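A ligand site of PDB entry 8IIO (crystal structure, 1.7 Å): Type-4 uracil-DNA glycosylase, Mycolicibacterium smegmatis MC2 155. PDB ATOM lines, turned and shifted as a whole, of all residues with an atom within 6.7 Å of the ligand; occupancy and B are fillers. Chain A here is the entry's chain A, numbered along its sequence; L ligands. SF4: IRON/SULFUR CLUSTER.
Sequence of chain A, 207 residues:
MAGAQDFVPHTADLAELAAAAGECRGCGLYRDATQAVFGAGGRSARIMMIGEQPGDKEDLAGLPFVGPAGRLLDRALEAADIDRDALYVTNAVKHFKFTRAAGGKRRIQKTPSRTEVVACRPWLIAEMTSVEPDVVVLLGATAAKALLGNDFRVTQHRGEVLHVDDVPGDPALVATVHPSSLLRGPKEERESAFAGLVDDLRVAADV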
ATOM      1  N   GLY A   3      25.747 -15.833 -25.474  1.00  0.00           N
ATOM      2  CA  GLY A   3      25.764 -14.411 -25.186  1.00  0.00           C
ATOM      3  C   GLY A   3      26.158 -14.110 -23.757  1.00  0.00           C
ATOM      4  O   GLY A   3      27.144 -14.640 -23.228  1.00  0.00           O
ATOM      5  N   ALA A   4      25.368 -13.244 -23.103  1.00  0.00           N
ATOM      6  CA  ALA A   4      25.656 -12.771 -21.757  1.00  0.00           C
ATOM      7  C   ALA A   4      25.265 -13.767 -20.664  1.00  0.00           C
ATOM      8  O   ALA A   4      25.476 -13.470 -19.489  1.00  0.00           O
ATOM      9  CB  ALA A   4      24.923 -11.442 -21.521  1.00  0.00           C
ATOM     10  N   PHE A   7      27.386 -14.539 -17.688  1.00  0.00           N
ATOM     11  CA  PHE A   7      27.833 -13.367 -16.962  1.00  0.00           C
ATOM     12  C   PHE A   7      26.778 -12.831 -15.996  1.00  0.00           C
ATOM     13  O   PHE A   7      27.096 -11.968 -15.181  1.00  0.00           O
ATOM     14  CB  PHE A   7      28.230 -12.261 -17.952  1.00  0.00           C
ATOM     15  CG  PHE A   7      29.436 -12.610 -18.768  1.00  0.00           C
ATOM     16  CD1 PHE A   7      30.708 -12.483 -18.247  1.00  0.00           C
ATOM     17  CD2 PHE A   7      29.291 -13.105 -20.057  1.00  0.00           C
ATOM     18  CE1 PHE A   7      31.826 -12.825 -18.995  1.00  0.00           C
ATOM     19  CE2 PHE A   7      30.400 -13.441 -20.828  1.00  0.00           C
ATOM     20  CZ  PHE A   7      31.665 -13.314 -20.286  1.00  0.00           C
ATOM     21  N   ALA A  21      27.156  -6.569 -14.872  1.00  0.00           N
ATOM     22  CA  ALA A  21      27.103  -6.146 -16.267  1.00  0.00           C
ATOM     23  C   ALA A  21      28.345  -5.357 -16.645  1.00  0.00           C
ATOM     24  O   ALA A  21      28.755  -5.376 -17.809  1.00  0.00           O
ATOM     25  CB  ALA A  21      25.849  -5.321 -16.528  1.00  0.00           C
ATOM     26  N   GLY A  22      28.950  -4.655 -15.681  1.00  0.00           N
ATOM     27  CA  GLY A  22      30.217  -3.988 -15.938  1.00  0.00           C
ATOM     28  C   GLY A  22      31.340  -4.930 -16.339  1.00  0.00           C
ATOM     29  O   GLY A  22      32.317  -4.489 -16.951  1.00  0.00           O
ATOM     30  N   GLU A  23      31.160  -6.214 -16.085  1.00  0.00           N
ATOM     31  CA  GLU A  23      32.209  -7.217 -16.411  1.00  0.00           C
ATOM     32  C   GLU A  23      31.770  -8.103 -17.587  1.00  0.00           C
ATOM     33  O   GLU A  23      32.472  -9.036 -17.895  1.00  0.00           O
ATOM     34  CB  GLU A  23      32.463  -8.139 -15.208  1.00  0.00           C
ATOM     35  CG  GLU A  23      32.824  -7.388 -13.947  1.00  0.00           C
ATOM     36  CD  GLU A  23      34.026  -6.476 -14.114  1.00  0.00           C
ATOM     37  OE1 GLU A  23      35.073  -6.960 -14.571  1.00  0.00           O
ATOM     38  N   CYS A  24      30.619  -7.798 -18.189  1.00  0.00           N
ATOM     39  CA  CYS A  24      30.094  -8.646 -19.259  1.00  0.00           C
ATOM     40  C   CYS A  24      30.967  -8.593 -20.502  1.00  0.00           C
ATOM     41  O   CYS A  24      31.423  -7.520 -20.919  1.00  0.00           O
ATOM     42  CB  CYS A  24      28.675  -8.207 -19.612  1.00  0.00           C
ATOM     43  SG  CYS A  24      27.827  -9.318 -20.763  1.00  0.00           S
ATOM     44  N   ARG A  25      31.202  -9.764 -21.095  1.00  0.00           N
ATOM     45  CA  ARG A  25      31.849  -9.901 -22.405  1.00  0.00           C
ATOM     46  C   ARG A  25      30.966 -10.703 -23.346  1.00  0.00           C
ATOM     47  O   ARG A  25      31.464 -11.362 -24.256  1.00  0.00           O
ATOM     48  CB  ARG A  25      33.223 -10.556 -22.271  1.00  0.00           C
ATOM     49  CG  ARG A  25      34.152  -9.850 -21.287  1.00  0.00           C
ATOM     50  CD  ARG A  25      35.577 -10.397 -21.361  1.00  0.00           C
ATOM     51  NE  ARG A  25      35.600 -11.865 -21.320  1.00  0.00           N
ATOM     52  CZ  ARG A  25      35.453 -12.574 -20.212  1.00  0.00           C
ATOM     53  NH1 ARG A  25      35.253 -11.998 -19.043  1.00  0.00           N
ATOM     54  NH2 ARG A  25      35.498 -13.899 -20.285  1.00  0.00           N
ATOM     55  N   GLY A  26      29.645 -10.639 -23.144  1.00  0.00           N
ATOM     56  CA  GLY A  26      28.701 -11.479 -23.869  1.00  0.00           C
ATOM     57  C   GLY A  26      28.643 -11.227 -25.363  1.00  0.00           C
ATOM     58  O   GLY A  26      28.140 -12.073 -26.102  1.00  0.00           O
ATOM     59  N   CYS A  27      29.122 -10.071 -25.821  1.00  0.00           N
ATOM     60  CA  CYS A  27      29.295  -9.790 -27.252  1.00  0.00           C
ATOM     61  C   CYS A  27      30.504  -8.871 -27.379  1.00  0.00           C
ATOM     62  O   CYS A  27      31.261  -8.678 -26.411  1.00  0.00           O
ATOM     63  CB  CYS A  27      28.011  -9.213 -27.864  1.00  0.00           C
ATOM     64  SG  CYS A  27      27.636  -7.472 -27.458  1.00  0.00           S
ATOM     65  N   GLY A  28      30.725  -8.318 -28.552  1.00  0.00           N
ATOM     66  CA  GLY A  28      31.922  -7.513 -28.718  1.00  0.00           C
ATOM     67  C   GLY A  28      31.801  -6.068 -28.286  1.00  0.00           C
ATOM     68  O   GLY A  28      32.812  -5.344 -28.298  1.00  0.00           O
ATOM     69  N   LEU A  29      30.613  -5.619 -27.892  1.00  0.00           N
ATOM     70  CA  LEU A  29      30.378  -4.178 -27.732  1.00  0.00           C
ATOM     71  C   LEU A  29      31.075  -3.606 -26.505  1.00  0.00           C
ATOM     72  O   LEU A  29      31.310  -2.385 -26.477  1.00  0.00           O
ATOM     73  CB  LEU A  29      28.888  -3.890 -27.671  1.00  0.00           C
ATOM     74  CG  LEU A  29      28.142  -4.209 -28.974  1.00  0.00           C
ATOM     75  CD1 LEU A  29      26.664  -3.862 -28.843  1.00  0.00           C
ATOM     76  CD2 LEU A  29      28.783  -3.440 -30.121  1.00  0.00           C
ATOM     77  N   TYR A  30      31.435  -4.440 -25.527  1.00  0.00           N
ATOM     78  CA  TYR A  30      32.115  -3.934 -24.342  1.00  0.00           C
ATOM     79  C   TYR A  30      33.487  -3.358 -24.664  1.00  0.00           C
ATOM     80  O   TYR A  30      33.997  -2.539 -23.894  1.00  0.00           O
ATOM     81  CB  TYR A  30      32.271  -5.050 -23.288  1.00  0.00           C
ATOM     82  CG  TYR A  30      33.379  -6.029 -23.613  1.00  0.00           C
ATOM     83  CD1 TYR A  30      33.141  -7.131 -24.433  1.00  0.00           C
ATOM     84  CD2 TYR A  30      34.667  -5.864 -23.101  1.00  0.00           C
ATOM     85  CE1 TYR A  30      34.151  -8.026 -24.737  1.00  0.00           C
ATOM     86  CE2 TYR A  30      35.680  -6.750 -23.395  1.00  0.00           C
ATOM     87  CZ  TYR A  30      35.418  -7.833 -24.214  1.00  0.00           C
ATOM     88  OH  TYR A  30      36.412  -8.722 -24.520  1.00  0.00           O
ATOM     89  N   ARG A  31      34.074  -3.798 -25.775  1.00  0.00           N
ATOM     90  CA  ARG A  31      35.488  -3.419 -26.031  1.00  0.00           C
ATOM     91  C   ARG A  31      35.674  -1.910 -26.254  1.00  0.00           C
ATOM     92  O   ARG A  31      36.559  -1.347 -25.634  1.00  0.00           O
ATOM     93  CB  ARG A  31      36.037  -4.201 -27.223  1.00  0.00           C
ATOM     94  CG  ARG A  31      35.980  -5.713 -27.081  1.00  0.00           C
ATOM     95  CD  ARG A  31      36.740  -6.406 -28.191  1.00  0.00           C
ATOM     96  N   ALA A  36      29.496  -0.393 -19.219  1.00  0.00           N
ATOM     97  CA  ALA A  36      28.123  -0.834 -19.366  1.00  0.00           C
ATOM     98  C   ALA A  36      27.201   0.197 -18.743  1.00  0.00           C
ATOM     99  O   ALA A  36      27.555   0.864 -17.773  1.00  0.00           O
ATOM    100  CB  ALA A  36      27.918  -2.202 -18.700  1.00  0.00           C
ATOM    101  N   ALA A  92      17.878  -2.405 -24.582  1.00  0.00           N
ATOM    102  CA  ALA A  92      17.999  -3.817 -25.006  1.00  0.00           C
ATOM    103  C   ALA A  92      19.477  -4.234 -25.007  1.00  0.00           C
ATOM    104  O   ALA A  92      19.734  -5.380 -24.700  1.00  0.00           O
ATOM    105  CB  ALA A  92      17.364  -3.991 -26.363  1.00  0.00           C
ATOM    106  N   VAL A  93      20.352  -3.328 -25.432  1.00  0.00           N
ATOM    107  CA  VAL A  93      21.827  -3.585 -25.362  1.00  0.00           C
ATOM    108  C   VAL A  93      22.433  -2.593 -24.366  1.00  0.00           C
ATOM    109  O   VAL A  93      21.952  -1.473 -24.297  1.00  0.00           O
ATOM    110  CB  VAL A  93      22.585  -3.694 -26.690  1.00  0.00           C
ATOM    111  CG1 VAL A  93      21.797  -4.506 -27.707  1.00  0.00           C
ATOM    112  CG2 VAL A  93      23.054  -2.382 -27.265  1.00  0.00           C
ATOM    113  N   LYS A  94      23.437  -3.053 -23.624  1.00  0.00           N
ATOM    114  CA  LYS A  94      23.956  -2.244 -22.498  1.00  0.00           C
ATOM    115  C   LYS A  94      25.302  -1.581 -22.765  1.00  0.00           C
ATOM    116  O   LYS A  94      25.769  -0.883 -21.893  1.00  0.00           O
ATOM    117  CB  LYS A  94      23.861  -3.038 -21.203  1.00  0.00           C
ATOM    118  CG  LYS A  94      22.436  -3.007 -20.672  1.00  0.00           C
ATOM    119  CD  LYS A  94      22.033  -4.173 -19.839  1.00  0.00           C
ATOM    120  CE  LYS A  94      20.683  -3.938 -19.219  1.00  0.00           C
ATOM    121  NZ  LYS A  94      19.584  -4.176 -20.184  1.00  0.00           N
ATOM    122  N   HIS A  95      25.842  -1.808 -23.954  1.00  0.00           N
ATOM    123  CA  HIS A  95      27.057  -1.061 -24.355  1.00  0.00           C
ATOM    124  C   HIS A  95      26.765  -0.267 -25.635  1.00  0.00           C
ATOM    125  O   HIS A  95      26.156  -0.809 -26.528  1.00  0.00           O
ATOM    126  CB  HIS A  95      28.289  -1.930 -24.562  1.00  0.00           C
ATOM    127  CG  HIS A  95      28.956  -2.334 -23.299  1.00  0.00           C
ATOM    128  ND1 HIS A  95      28.726  -3.534 -22.728  1.00  0.00           N
ATOM    129  CD2 HIS A  95      29.851  -1.718 -22.515  1.00  0.00           C
ATOM    130  CE1 HIS A  95      29.450  -3.683 -21.640  1.00  0.00           C
ATOM    131  NE2 HIS A  95      30.145  -2.569 -21.494  1.00  0.00           N
ATOM    132  N   PHE A  96      27.239   0.969 -25.651  1.00  0.00           N
ATOM    133  CA  PHE A  96      27.066   1.849 -26.829  1.00  0.00           C
ATOM    134  C   PHE A  96      27.851   1.298 -28.023  1.00  0.00           C
ATOM    135  O   PHE A  96      29.018   1.000 -27.877  1.00  0.00           O
ATOM    136  CB  PHE A  96      27.533   3.251 -26.409  1.00  0.00           C
ATOM    137  CG  PHE A  96      27.594   4.333 -27.456  1.00  0.00           C
ATOM    138  CD1 PHE A  96      26.564   4.514 -28.358  1.00  0.00           C
ATOM    139  CD2 PHE A  96      28.658   5.207 -27.472  1.00  0.00           C
ATOM    140  CE1 PHE A  96      26.625   5.537 -29.295  1.00  0.00           C
ATOM    141  CE2 PHE A  96      28.719   6.230 -28.408  1.00  0.00           C
ATOM    142  CZ  PHE A  96      27.702   6.395 -29.320  1.00  0.00           C
ATOM    143  N   GLU A 116      23.622  -9.287 -31.367  1.00  0.00           N
ATOM    144  CA  GLU A 116      24.001  -8.528 -30.138  1.00  0.00           C
ATOM    145  C   GLU A 116      22.770  -8.381 -29.231  1.00  0.00           C
ATOM    146  O   GLU A 116      22.891  -8.513 -28.036  1.00  0.00           O
ATOM    147  CB  GLU A 116      24.624  -7.187 -30.530  1.00  0.00           C
ATOM    148  CG  GLU A 116      25.996  -7.321 -31.150  1.00  0.00           C
ATOM    149  CD  GLU A 116      26.475  -6.179 -32.049  1.00  0.00           C
ATOM    150  OE1 GLU A 116      25.641  -5.416 -32.520  1.00  0.00           O
ATOM    151  OE2 GLU A 116      27.689  -6.075 -32.256  1.00  0.00           O
ATOM    152  N   ALA A 119      22.248 -11.585 -27.598  1.00  0.00           N
ATOM    153  CA  ALA A 119      23.349 -11.845 -26.645  1.00  0.00           C
ATOM    154  C   ALA A 119      23.088 -11.086 -25.349  1.00  0.00           C
ATOM    155  O   ALA A 119      23.386 -11.627 -24.305  1.00  0.00           O
ATOM    156  CB  ALA A 119      24.653 -11.380 -27.245  1.00  0.00           C
ATOM    157  N   CYS A 120      22.533  -9.887 -25.464  1.00  0.00           N
ATOM    158  CA  CYS A 120      22.364  -9.009 -24.262  1.00  0.00           C
ATOM    159  C   CYS A 120      21.044  -9.275 -23.553  1.00  0.00           C
ATOM    160  O   CYS A 120      20.886  -8.881 -22.417  1.00  0.00           O
ATOM    161  CB  CYS A 120      22.390  -7.547 -24.689  1.00  0.00           C
ATOM    162  SG  CYS A 120      22.965  -6.490 -23.326  1.00  0.00           S
ATOM    163  N   ARG A 121      20.141  -9.961 -24.253  1.00  0.00           N
ATOM    164  CA  ARG A 121      18.788 -10.201 -23.713  1.00  0.00           C
ATOM    165  C   ARG A 121      18.788 -10.818 -22.304  1.00  0.00           C
ATOM    166  O   ARG A 121      17.879 -10.497 -21.547  1.00  0.00           O
ATOM    167  CB  ARG A 121      17.904 -10.969 -24.713  1.00  0.00           C
ATOM    168  CG  ARG A 121      16.428 -10.870 -24.410  1.00  0.00           C
ATOM    169  CD  ARG A 121      15.589 -11.407 -25.542  1.00  0.00           C
ATOM    170  NE  ARG A 121      16.048 -12.708 -25.967  1.00  0.00           N
ATOM    171  CZ  ARG A 121      15.724 -13.256 -27.138  1.00  0.00           C
ATOM    172  NH1 ARG A 121      14.947 -12.582 -27.971  1.00  0.00           N
ATOM    173  NH2 ARG A 121      16.174 -14.448 -27.455  1.00  0.00           N
ATOM    174  N   PRO A 122      19.688 -11.745 -21.939  1.00  0.00           N
ATOM    175  CA  PRO A 122      19.720 -12.224 -20.554  1.00  0.00           C
ATOM    176  C   PRO A 122      19.676 -11.130 -19.474  1.00  0.00           C
ATOM    177  O   PRO A 122      19.091 -11.347 -18.476  1.00  0.00           O
ATOM    178  CB  PRO A 122      21.009 -13.057 -20.490  1.00  0.00           C
ATOM    179  CG  PRO A 122      21.118 -13.632 -21.867  1.00  0.00           C
ATOM    180  CD  PRO A 122      20.597 -12.548 -22.770  1.00  0.00           C
ATOM    181  N   TRP A 123      20.312  -9.981 -19.729  1.00  0.00           N
ATOM    182  CA  TRP A 123      20.239  -8.866 -18.744  1.00  0.00           C
ATOM    183  C   TRP A 123      18.812  -8.340 -18.661  1.00  0.00           C
ATOM    184  O   TRP A 123      18.371  -8.054 -17.581  1.00  0.00           O
ATOM    185  CB  TRP A 123      21.220  -7.748 -19.118  1.00  0.00           C
ATOM    186  CG  TRP A 123      22.651  -8.155 -18.999  1.00  0.00           C
ATOM    187  CD1 TRP A 123      23.553  -8.298 -19.999  1.00  0.00           C
ATOM    188  CD2 TRP A 123      23.327  -8.495 -17.777  1.00  0.00           C
ATOM    189  NE1 TRP A 123      24.760  -8.698 -19.494  1.00  0.00           N
ATOM    190  CE2 TRP A 123      24.655  -8.835 -18.133  1.00  0.00           C
ATOM    191  CE3 TRP A 123      22.963  -8.551 -16.424  1.00  0.00           C
ATOM    192  CZ2 TRP A 123      25.598  -9.229 -17.190  1.00  0.00           C
ATOM    193  CZ3 TRP A 123      23.900  -8.929 -15.494  1.00  0.00           C
ATOM    194  CH2 TRP A 123      25.194  -9.262 -15.875  1.00  0.00           C
HETATM  195 FE1  SF4 L   1      25.232  -6.614 -23.513  1.00  0.00          FE
HETATM  196 FE2  SF4 L   1      27.262  -7.283 -25.197  1.00  0.00          FE
HETATM  197 FE3  SF4 L   1      27.375  -7.925 -22.521  1.00  0.00          FE
HETATM  198 FE4  SF4 L   1      27.617  -5.338 -23.372  1.00  0.00          FE
HETATM  199  S1  SF4 L   1      29.076  -7.069 -23.825  1.00  0.00           S
HETATM  200  S2  SF4 L   1      26.347  -6.076 -21.599  1.00  0.00           S
HETATM  201  S3  SF4 L   1      26.178  -5.283 -25.120  1.00  0.00           S
HETATM  202  S4  SF4 L   1      25.917  -8.728 -24.053  1.00  0.00           S
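The backbone carbonyl oxygen of Ala 119 sits at hydrogen-bond distance from the backbone NH of Ala 4 (2.8 Å).
The side-chain sulfur of Cys 120 lies close to the backbone NH of Lys 94.
The side-chain sulfur (SG) of Cys 24 sits close to the indole nitrogen (NE1) of Trp 123 (3.4 Å).
The backbone carbonyl oxygen (O) of Ala 92 lies close to the side-chain sulfur (SG) of Cys 120, 3.7 Å away.
The backbone NH (N) of Ala 36 is in hydrogen-bond range of a ring nitrogen (NE2) of His 95, 3.2 Å away.
The side-chain sulfur of Cys 24 sits close to the backbone NH of Gly 26 (3.3 Å).
SG of Cys 27 lies close to N of Leu 29, 3.5 Å away.
A sulfur (S2) of the ligand sits close to the indole nitrogen (NE1) of Trp 123 (3.7 Å).
The side-chain sulfur of Cys 24 binds an iron atom (FE3) of the ligand (2.3 Å).
A ring nitrogen (ND1) of His 95 binds an iron atom (FE4) of the ligand (2.2 Å).
FE2 of the ligand is bound by SG of Cys 27, 2.3 Å away.
A sulfur (S1) of the ligand sits close to the backbone NH of Gly 26, 3.7 Å away.
A sulfur (S1) of the ligand lies close to the backbone NH (N) of Cys 27.
N of His 95 lies close to S3 of the ligand (3.7 Å).
FE1 of the ligand is bound by SG of Cys 120 (2.3 Å).
Residues that only touch the ligand: Ala 4, Leu 29, Tyr 30, Lys 94 and Ala 119.
Hydrophobic or aromatic side chains within 4 Å of the ligand: Ala 4, Leu 29, Tyr 30, His 95 and Trp 123.
11 residues have an atom within 4 Å of the ligand: Ala 4, Cys 24, Gly 26, Cys 27, Leu 29, Tyr 30, Lys 94, His 95, Ala 119, Cys 120 and Trp 123.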
